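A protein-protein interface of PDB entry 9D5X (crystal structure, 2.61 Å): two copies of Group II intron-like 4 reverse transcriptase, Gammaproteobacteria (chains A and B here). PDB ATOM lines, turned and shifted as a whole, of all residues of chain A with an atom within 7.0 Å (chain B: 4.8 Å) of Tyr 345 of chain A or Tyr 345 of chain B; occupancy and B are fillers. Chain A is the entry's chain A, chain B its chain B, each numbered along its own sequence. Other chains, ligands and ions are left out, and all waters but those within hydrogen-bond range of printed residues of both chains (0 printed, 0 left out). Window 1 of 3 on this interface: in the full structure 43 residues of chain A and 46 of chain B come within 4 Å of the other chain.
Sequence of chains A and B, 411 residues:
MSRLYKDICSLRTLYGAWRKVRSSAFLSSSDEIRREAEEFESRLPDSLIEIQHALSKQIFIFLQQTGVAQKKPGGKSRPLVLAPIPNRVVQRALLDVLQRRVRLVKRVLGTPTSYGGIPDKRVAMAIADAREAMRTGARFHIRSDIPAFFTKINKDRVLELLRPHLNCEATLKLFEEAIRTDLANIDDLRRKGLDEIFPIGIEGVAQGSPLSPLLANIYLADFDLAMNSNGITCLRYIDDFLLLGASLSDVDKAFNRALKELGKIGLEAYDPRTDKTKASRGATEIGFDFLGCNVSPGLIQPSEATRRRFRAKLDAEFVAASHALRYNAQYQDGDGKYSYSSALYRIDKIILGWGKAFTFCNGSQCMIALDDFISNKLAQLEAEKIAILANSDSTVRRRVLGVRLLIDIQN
Among the printed residues, pairs that only touch across the chains: Gly 402 of chain A with Asp 348 of chain B (3.3 Å), Leu 344 of chain A with Ser 341 of chain B (3.5 Å), Ser 341 of chain A with Leu 344 of chain B (3.5 Å), Val 403 of chain A with Asp 348 of chain B (3.6 Å), Ser 342 of chain A with Tyr 345 of chain B (3.7 Å), Arg 404 of chain A with Lys 349 of chain B (3.8 Å), Tyr 345 of chain A with Ser 342 of chain B (3.8 Å), Tyr 345 of chain A with Tyr 345 of chain B (3.8 Å), Gly 402 of chain A with Leu 344 of chain B (3.9 Å), Ser 341 of chain A with Ser 341 of chain B (3.9 Å) and Val 403 of chain A with Leu 344 of chain B (3.9 Å).
Of the 9 printed residues of chain B, 6 touch a printed residue of chain A. Hydrophobic or aromatic side chains of chain B within 4 Å of the printed part of chain A: Leu 344 and Tyr 345. Among the printed residues, 12 pairs touch across the chains.
The side-chain carboxylate (OD2) of Asp 348 of chain B lies within salt-bridge range of the guanidinium group (NH2) of Arg 404 of chain A, 2.7 Å away.
OG of Ser 339 of chain A lies within hydrogen-bond range of OG of Ser 342 of chain A, 3.4 Å away. The side-chain hydroxyl of Ser 341 of chain A sits at hydrogen-bond distance from the backbone carbonyl oxygen of Leu 401 of chain A (2.9 Å). The side-chain hydroxyl (OG) of Ser 341 of chain A is in hydrogen-bond range of the backbone carbonyl oxygen (O) of Gly 402 of chain A. The side-chain amino group (NZ) of Lys 349 of chain A is in hydrogen-bond range of the backbone carbonyl oxygen (O) of Tyr 345 of chain A. The backbone carbonyl oxygen (O) of Tyr 345 of chain B sits at hydrogen-bond distance from the side-chain amino group (NZ) of Lys 349 of chain B, at 3.1 Å. The side-chain carboxylate (OD2) of Asp 348 of chain B lies within salt-bridge range of the side-chain amino group (NZ) of Lys 349 of chain B (2.6 Å).
Ser 341 of chain A touches its own counterpart, Ser 341 of chain B. Ser 341 of chain A touches Leu 344 of chain B, and with the chains exchanged Leu 344 of chain A touches Ser 341 of chain B. Ser 342 of chain A touches Tyr 345 of chain B, and with the chains exchanged Tyr 345 of chain A touches Ser 342 of chain B. Tyr 345 of chain B touches its own counterpart, Tyr 345 of chain A. 9 positions are printed for both chains.
Of the printed residues of chain B, Ser 342 of chain A touches Tyr 345 (3.7 Å). Tyr 345 of chain A touches two residues of chain B. Printed residues of chain B within 4 Å of Gly 402 of chain A: Leu 344 (3.9 Å) and Asp 348 (3.3 Å). Of the printed residues of chain B, Arg 404 of chain A touches Asp 348 (2.7 Å) and Lys 349 (3.8 Å). Tyr 345 of chain B touches two residues of chain A. The nearest residue of chain A that does not touch Tyr 345 of chain B is Ser 341 of chain A (4.2 Å). The nearest printed residue of chain B that does not touch Val 403 of chain A is Ile 347 of chain B (4.6 Å).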
ATOM      1  N   GLY A 336      12.643  25.003 -21.866  1.00  0.00           N
ATOM      2  CA  GLY A 336      12.564  25.679 -20.588  1.00  0.00           C
ATOM      3  C   GLY A 336      11.332  26.551 -20.512  1.00  0.00           C
ATOM      4  O   GLY A 336      10.796  26.790 -19.426  1.00  0.00           O
ATOM      5  N   LYS A 337      10.879  27.030 -21.673  1.00  0.00           N
ATOM      6  CA  LYS A 337       9.664  27.837 -21.728  1.00  0.00           C
ATOM      7  C   LYS A 337       8.455  27.072 -21.206  1.00  0.00           C
ATOM      8  O   LYS A 337       7.575  27.660 -20.563  1.00  0.00           O
ATOM      9  CB  LYS A 337       9.410  28.309 -23.162  1.00  0.00           C
ATOM     10  CG  LYS A 337       8.074  29.020 -23.377  1.00  0.00           C
ATOM     11  CD  LYS A 337       7.829  29.291 -24.852  1.00  0.00           C
ATOM     12  CE  LYS A 337       6.472  29.935 -25.082  1.00  0.00           C
ATOM     13  NZ  LYS A 337       6.183  30.106 -26.532  1.00  0.00           N
ATOM     14  N   SER A 339       8.741  24.203 -19.233  1.00  0.00           N
ATOM     15  CA  SER A 339       9.064  23.405 -18.062  1.00  0.00           C
ATOM     16  C   SER A 339       7.972  23.571 -17.003  1.00  0.00           C
ATOM     17  O   SER A 339       7.125  24.464 -17.081  1.00  0.00           O
ATOM     18  CB  SER A 339      10.426  23.807 -17.502  1.00  0.00           C
ATOM     19  OG  SER A 339      10.440  25.172 -17.123  1.00  0.00           O
ATOM     20  N   TYR A 340       8.001  22.693 -15.998  1.00  0.00           N
ATOM     21  CA  TYR A 340       6.902  22.632 -15.037  1.00  0.00           C
ATOM     22  C   TYR A 340       6.687  23.974 -14.348  1.00  0.00           C
ATOM     23  O   TYR A 340       5.551  24.446 -14.223  1.00  0.00           O
ATOM     24  CB  TYR A 340       7.156  21.534 -14.006  1.00  0.00           C
ATOM     25  CG  TYR A 340       6.005  21.357 -13.040  1.00  0.00           C
ATOM     26  CD1 TYR A 340       4.829  20.738 -13.442  1.00  0.00           C
ATOM     27  CD2 TYR A 340       6.092  21.812 -11.733  1.00  0.00           C
ATOM     28  CE1 TYR A 340       3.772  20.576 -12.567  1.00  0.00           C
ATOM     29  CE2 TYR A 340       5.039  21.655 -10.848  1.00  0.00           C
ATOM     30  CZ  TYR A 340       3.882  21.036 -11.273  1.00  0.00           C
ATOM     31  OH  TYR A 340       2.830  20.875 -10.401  1.00  0.00           O
ATOM     32  N   SER A 341       7.769  24.613 -13.898  1.00  0.00           N
ATOM     33  CA  SER A 341       7.625  25.901 -13.226  1.00  0.00           C
ATOM     34  C   SER A 341       7.225  26.995 -14.208  1.00  0.00           C
ATOM     35  O   SER A 341       6.354  27.820 -13.906  1.00  0.00           O
ATOM     36  CB  SER A 341       8.922  26.275 -12.507  1.00  0.00           C
ATOM     37  OG  SER A 341       9.970  26.513 -13.428  1.00  0.00           O
ATOM     38  N   SER A 342       7.847  27.018 -15.389  1.00  0.00           N
ATOM     39  CA  SER A 342       7.515  28.046 -16.370  1.00  0.00           C
ATOM     40  C   SER A 342       6.105  27.869 -16.918  1.00  0.00           C
ATOM     41  O   SER A 342       5.425  28.859 -17.199  1.00  0.00           O
ATOM     42  CB  SER A 342       8.534  28.039 -17.509  1.00  0.00           C
ATOM     43  OG  SER A 342       9.800  28.492 -17.069  1.00  0.00           O
ATOM     44  N   ALA A 343       5.647  26.624 -17.068  1.00  0.00           N
ATOM     45  CA  ALA A 343       4.304  26.391 -17.588  1.00  0.00           C
ATOM     46  C   ALA A 343       3.245  26.846 -16.593  1.00  0.00           C
ATOM     47  O   ALA A 343       2.289  27.537 -16.963  1.00  0.00           O
ATOM     48  CB  ALA A 343       4.118  24.913 -17.932  1.00  0.00           C
ATOM     49  N   LEU A 344       3.396  26.462 -15.323  1.00  0.00           N
ATOM     50  CA  LEU A 344       2.482  26.945 -14.294  1.00  0.00           C
ATOM     51  C   LEU A 344       2.533  28.461 -14.175  1.00  0.00           C
ATOM     52  O   LEU A 344       1.530  29.093 -13.824  1.00  0.00           O
ATOM     53  CB  LEU A 344       2.810  26.302 -12.946  1.00  0.00           C
ATOM     54  CG  LEU A 344       2.080  25.024 -12.526  1.00  0.00           C
ATOM     55  CD1 LEU A 344       2.386  23.875 -13.469  1.00  0.00           C
ATOM     56  CD2 LEU A 344       2.447  24.654 -11.096  1.00  0.00           C
ATOM     57  N   TYR A 345       3.688  29.060 -14.466  1.00  0.00           N
ATOM     58  CA  TYR A 345       3.820  30.507 -14.372  1.00  0.00           C
ATOM     59  C   TYR A 345       3.031  31.203 -15.474  1.00  0.00           C
ATOM     60  O   TYR A 345       2.243  32.116 -15.205  1.00  0.00           O
ATOM     61  CB  TYR A 345       5.298  30.895 -14.433  1.00  0.00           C
ATOM     62  CG  TYR A 345       5.572  32.363 -14.205  1.00  0.00           C
ATOM     63  CD1 TYR A 345       5.756  32.864 -12.923  1.00  0.00           C
ATOM     64  CD2 TYR A 345       5.655  33.248 -15.273  1.00  0.00           C
ATOM     65  CE1 TYR A 345       6.011  34.206 -12.708  1.00  0.00           C
ATOM     66  CE2 TYR A 345       5.909  34.591 -15.070  1.00  0.00           C
ATOM     67  CZ  TYR A 345       6.087  35.065 -13.786  1.00  0.00           C
ATOM     68  OH  TYR A 345       6.340  36.403 -13.582  1.00  0.00           O
ATOM     69  N   ARG A 346       3.228  30.783 -16.726  1.00  0.00           N
ATOM     70  CA  ARG A 346       2.540  31.435 -17.837  1.00  0.00           C
ATOM     71  C   ARG A 346       1.042  31.157 -17.805  1.00  0.00           C
ATOM     72  O   ARG A 346       0.238  32.046 -18.108  1.00  0.00           O
ATOM     73  CB  ARG A 346       3.149  30.995 -19.170  1.00  0.00           C
ATOM     74  CG  ARG A 346       3.280  29.491 -19.349  1.00  0.00           C
ATOM     75  CD  ARG A 346       4.201  29.140 -20.513  1.00  0.00           C
ATOM     76  NE  ARG A 346       3.533  29.254 -21.804  1.00  0.00           N
ATOM     77  CZ  ARG A 346       3.584  30.322 -22.588  1.00  0.00           C
ATOM     78  NH1 ARG A 346       4.267  31.401 -22.244  1.00  0.00           N
ATOM     79  NH2 ARG A 346       2.932  30.306 -23.747  1.00  0.00           N
ATOM     80  N   ILE A 347       0.648  29.934 -17.439  1.00  0.00           N
ATOM     81  CA  ILE A 347      -0.775  29.622 -17.317  1.00  0.00           C
ATOM     82  C   ILE A 347      -1.422  30.518 -16.272  1.00  0.00           C
ATOM     83  O   ILE A 347      -2.539  31.017 -16.464  1.00  0.00           O
ATOM     84  CB  ILE A 347      -0.972  28.130 -16.989  1.00  0.00           C
ATOM     85  CG1 ILE A 347      -0.625  27.263 -18.200  1.00  0.00           C
ATOM     86  CG2 ILE A 347      -2.399  27.860 -16.528  1.00  0.00           C
ATOM     87  CD1 ILE A 347      -0.596  25.778 -17.899  1.00  0.00           C
ATOM     88  N   ASP A 348      -0.726  30.750 -15.157  1.00  0.00           N
ATOM     89  CA  ASP A 348      -1.223  31.673 -14.141  1.00  0.00           C
ATOM     90  C   ASP A 348      -1.487  33.050 -14.735  1.00  0.00           C
ATOM     91  O   ASP A 348      -2.530  33.661 -14.475  1.00  0.00           O
ATOM     92  CB  ASP A 348      -0.223  31.768 -12.987  1.00  0.00           C
ATOM     93  CG  ASP A 348      -0.601  32.836 -11.978  1.00  0.00           C
ATOM     94  OD1 ASP A 348      -1.635  32.673 -11.299  1.00  0.00           O
ATOM     95  OD2 ASP A 348       0.137  33.840 -11.869  1.00  0.00           O
ATOM     96  N   LYS A 349      -0.551  33.554 -15.544  1.00  0.00           N
ATOM     97  CA  LYS A 349      -0.733  34.867 -16.152  1.00  0.00           C
ATOM     98  C   LYS A 349      -1.811  34.846 -17.228  1.00  0.00           C
ATOM     99  O   LYS A 349      -2.538  35.832 -17.393  1.00  0.00           O
ATOM    100  CB  LYS A 349       0.592  35.367 -16.726  1.00  0.00           C
ATOM    101  CG  LYS A 349       1.721  35.390 -15.706  1.00  0.00           C
ATOM    102  CD  LYS A 349       1.293  36.095 -14.424  1.00  0.00           C
ATOM    103  CE  LYS A 349       2.331  35.924 -13.325  1.00  0.00           C
ATOM    104  NZ  LYS A 349       2.479  34.500 -12.911  1.00  0.00           N
ATOM    105  N   ILE A 350      -1.931  33.739 -17.968  1.00  0.00           N
ATOM    106  CA  ILE A 350      -3.024  33.600 -18.927  1.00  0.00           C
ATOM    107  C   ILE A 350      -4.367  33.689 -18.215  1.00  0.00           C
ATOM    108  O   ILE A 350      -5.303  34.337 -18.696  1.00  0.00           O
ATOM    109  CB  ILE A 350      -2.883  32.282 -19.712  1.00  0.00           C
ATOM    110  CG1 ILE A 350      -1.707  32.362 -20.688  1.00  0.00           C
ATOM    111  CG2 ILE A 350      -4.174  31.951 -20.453  1.00  0.00           C
ATOM    112  CD1 ILE A 350      -1.488  31.096 -21.484  1.00  0.00           C
ATOM    113  N   LEU A 401      11.589  20.297 -13.779  1.00  0.00           N
ATOM    114  CA  LEU A 401      10.980  21.324 -12.940  1.00  0.00           C
ATOM    115  C   LEU A 401      11.251  22.736 -13.438  1.00  0.00           C
ATOM    116  O   LEU A 401      10.492  23.649 -13.099  1.00  0.00           O
ATOM    117  CB  LEU A 401      11.465  21.187 -11.496  1.00  0.00           C
ATOM    118  CG  LEU A 401      10.886  20.013 -10.707  1.00  0.00           C
ATOM    119  CD1 LEU A 401      11.529  19.920  -9.334  1.00  0.00           C
ATOM    120  CD2 LEU A 401       9.377  20.150 -10.585  1.00  0.00           C
ATOM    121  N   GLY A 402      12.304  22.941 -14.223  1.00  0.00           N
ATOM    122  CA  GLY A 402      12.575  24.254 -14.771  1.00  0.00           C
ATOM    123  C   GLY A 402      13.526  25.088 -13.940  1.00  0.00           C
ATOM    124  O   GLY A 402      13.316  26.293 -13.765  1.00  0.00           O
ATOM    125  N   VAL A 403      14.577  24.460 -13.421  1.00  0.00           N
ATOM    126  CA  VAL A 403      15.626  25.147 -12.675  1.00  0.00           C
ATOM    127  C   VAL A 403      16.948  24.790 -13.340  1.00  0.00           C
ATOM    128  O   VAL A 403      17.444  23.667 -13.183  1.00  0.00           O
ATOM    129  CB  VAL A 403      15.631  24.770 -11.189  1.00  0.00           C
ATOM    130  CG1 VAL A 403      16.808  25.412 -10.490  1.00  0.00           C
ATOM    131  CG2 VAL A 403      14.327  25.197 -10.532  1.00  0.00           C
ATOM    132  N   ARG A 404      17.516  25.744 -14.077  1.00  0.00           N
ATOM    133  CA  ARG A 404      18.692  25.511 -14.905  1.00  0.00           C
ATOM    134  C   ARG A 404      19.861  24.972 -14.084  1.00  0.00           C
ATOM    135  O   ARG A 404      19.939  25.146 -12.864  1.00  0.00           O
ATOM    136  CB  ARG A 404      19.117  26.804 -15.596  1.00  0.00           C
ATOM    137  CG  ARG A 404      18.987  26.799 -17.107  1.00  0.00           C
ATOM    138  CD  ARG A 404      19.343  28.166 -17.665  1.00  0.00           C
ATOM    139  NE  ARG A 404      18.413  29.191 -17.206  1.00  0.00           N
ATOM    140  CZ  ARG A 404      17.385  29.636 -17.914  1.00  0.00           C
ATOM    141  NH1 ARG A 404      17.141  29.187 -19.133  1.00  0.00           N
ATOM    142  NH2 ARG A 404      16.582  30.555 -17.386  1.00  0.00           N
ATOM    143  N   SER B 341       5.322  27.871  -8.213  1.00  0.00           N
ATOM    144  CA  SER B 341       5.672  28.121  -9.607  1.00  0.00           C
ATOM    145  C   SER B 341       6.494  29.395  -9.751  1.00  0.00           C
ATOM    146  O   SER B 341       7.460  29.431 -10.522  1.00  0.00           O
ATOM    147  CB  SER B 341       4.410  28.203 -10.465  1.00  0.00           C
ATOM    148  OG  SER B 341       3.573  29.266 -10.050  1.00  0.00           O
ATOM    149  N   SER B 342       6.129  30.450  -9.019  1.00  0.00           N
ATOM    150  CA  SER B 342       6.862  31.707  -9.131  1.00  0.00           C
ATOM    151  C   SER B 342       8.261  31.591  -8.538  1.00  0.00           C
ATOM    152  O   SER B 342       9.228  32.091  -9.122  1.00  0.00           O
ATOM    153  CB  SER B 342       6.089  32.834  -8.452  1.00  0.00           C
ATOM    154  OG  SER B 342       4.935  33.185  -9.193  1.00  0.00           O
ATOM    155  N   ALA B 343       8.386  30.937  -7.380  1.00  0.00           N
ATOM    156  CA  ALA B 343       9.691  30.811  -6.737  1.00  0.00           C
ATOM    157  C   ALA B 343      10.661  30.026  -7.611  1.00  0.00           C
ATOM    158  O   ALA B 343      11.780  30.477  -7.877  1.00  0.00           O
ATOM    159  CB  ALA B 343       9.543  30.152  -5.365  1.00  0.00           C
ATOM    160  N   LEU B 344      10.243  28.842  -8.073  1.00  0.00           N
ATOM    161  CA  LEU B 344      11.084  28.067  -8.981  1.00  0.00           C
ATOM    162  C   LEU B 344      11.392  28.843 -10.255  1.00  0.00           C
ATOM    163  O   LEU B 344      12.461  28.663 -10.850  1.00  0.00           O
ATOM    164  CB  LEU B 344      10.410  26.737  -9.321  1.00  0.00           C
ATOM    165  CG  LEU B 344      10.795  25.513  -8.488  1.00  0.00           C
ATOM    166  CD1 LEU B 344      10.389  25.691  -7.036  1.00  0.00           C
ATOM    167  CD2 LEU B 344      10.175  24.253  -9.071  1.00  0.00           C
ATOM    168  N   TYR B 345      10.476  29.712 -10.682  1.00  0.00           N
ATOM    169  CA  TYR B 345      10.713  30.522 -11.870  1.00  0.00           C
ATOM    170  C   TYR B 345      11.770  31.589 -11.609  1.00  0.00           C
ATOM    171  O   TYR B 345      12.664  31.800 -12.437  1.00  0.00           O
ATOM    172  CB  TYR B 345       9.400  31.156 -12.330  1.00  0.00           C
ATOM    173  CG  TYR B 345       9.512  32.013 -13.569  1.00  0.00           C
ATOM    174  CD1 TYR B 345       9.428  31.450 -14.834  1.00  0.00           C
ATOM    175  CD2 TYR B 345       9.683  33.388 -13.472  1.00  0.00           C
ATOM    176  CE1 TYR B 345       9.525  32.231 -15.972  1.00  0.00           C
ATOM    177  CE2 TYR B 345       9.780  34.176 -14.600  1.00  0.00           C
ATOM    178  CZ  TYR B 345       9.701  33.595 -15.847  1.00  0.00           C
ATOM    179  OH  TYR B 345       9.797  34.380 -16.972  1.00  0.00           O
ATOM    180  N   ARG B 346      11.691  32.265 -10.463  1.00  0.00           N
ATOM    181  CA  ARG B 346      12.645  33.327 -10.164  1.00  0.00           C
ATOM    182  C   ARG B 346      14.010  32.768  -9.779  1.00  0.00           C
ATOM    183  O   ARG B 346      15.042  33.343 -10.142  1.00  0.00           O
ATOM    184  CB  ARG B 346      12.097  34.224  -9.054  1.00  0.00           C
ATOM    185  CG  ARG B 346      13.015  35.370  -8.655  1.00  0.00           C
ATOM    186  CD  ARG B 346      12.406  36.217  -7.543  1.00  0.00           C
ATOM    187  NE  ARG B 346      11.999  35.404  -6.402  1.00  0.00           N
ATOM    188  CZ  ARG B 346      10.754  35.005  -6.174  1.00  0.00           C
ATOM    189  NH1 ARG B 346       9.758  35.355  -6.971  1.00  0.00           N
ATOM    190  NH2 ARG B 346      10.506  34.227  -5.124  1.00  0.00           N
ATOM    191  N   ILE B 347      14.035  31.652  -9.046  1.00  0.00           N
ATOM    192  CA  ILE B 347      15.305  31.016  -8.706  1.00  0.00           C
ATOM    193  C   ILE B 347      16.039  30.589  -9.972  1.00  0.00           C
ATOM    194  O   ILE B 347      17.268  30.702 -10.065  1.00  0.00           O
ATOM    195  CB  ILE B 347      15.071  29.828  -7.753  1.00  0.00           C
ATOM    196  CG1 ILE B 347      14.574  30.325  -6.395  1.00  0.00           C
ATOM    197  CG2 ILE B 347      16.343  29.009  -7.588  1.00  0.00           C
ATOM    198  CD1 ILE B 347      14.231  29.213  -5.427  1.00  0.00           C
ATOM    199  N   ASP B 348      15.292  30.105 -10.968  1.00  0.00           N
ATOM    200  CA  ASP B 348      15.896  29.746 -12.247  1.00  0.00           C
ATOM    201  C   ASP B 348      16.581  30.946 -12.890  1.00  0.00           C
ATOM    202  O   ASP B 348      17.690  30.824 -13.424  1.00  0.00           O
ATOM    203  CB  ASP B 348      14.828  29.174 -13.179  1.00  0.00           C
ATOM    204  CG  ASP B 348      15.347  28.934 -14.582  1.00  0.00           C
ATOM    205  OD1 ASP B 348      16.214  28.053 -14.754  1.00  0.00           O
ATOM    206  OD2 ASP B 348      14.883  29.624 -15.515  1.00  0.00           O
ATOM    207  N   LYS B 349      15.940  32.116 -12.840  1.00  0.00           N
ATOM    208  CA  LYS B 349      16.530  33.304 -13.446  1.00  0.00           C
ATOM    209  C   LYS B 349      17.718  33.807 -12.637  1.00  0.00           C
ATOM    210  O   LYS B 349      18.694  34.313 -13.206  1.00  0.00           O
ATOM    211  CB  LYS B 349      15.470  34.396 -13.594  1.00  0.00           C
ATOM    212  CG  LYS B 349      14.230  33.940 -14.341  1.00  0.00           C
ATOM    213  CD  LYS B 349      14.597  33.298 -15.674  1.00  0.00           C
ATOM    214  CE  LYS B 349      13.402  32.598 -16.308  1.00  0.00           C
ATOM    215  NZ  LYS B 349      12.962  31.415 -15.519  1.00  0.00           N
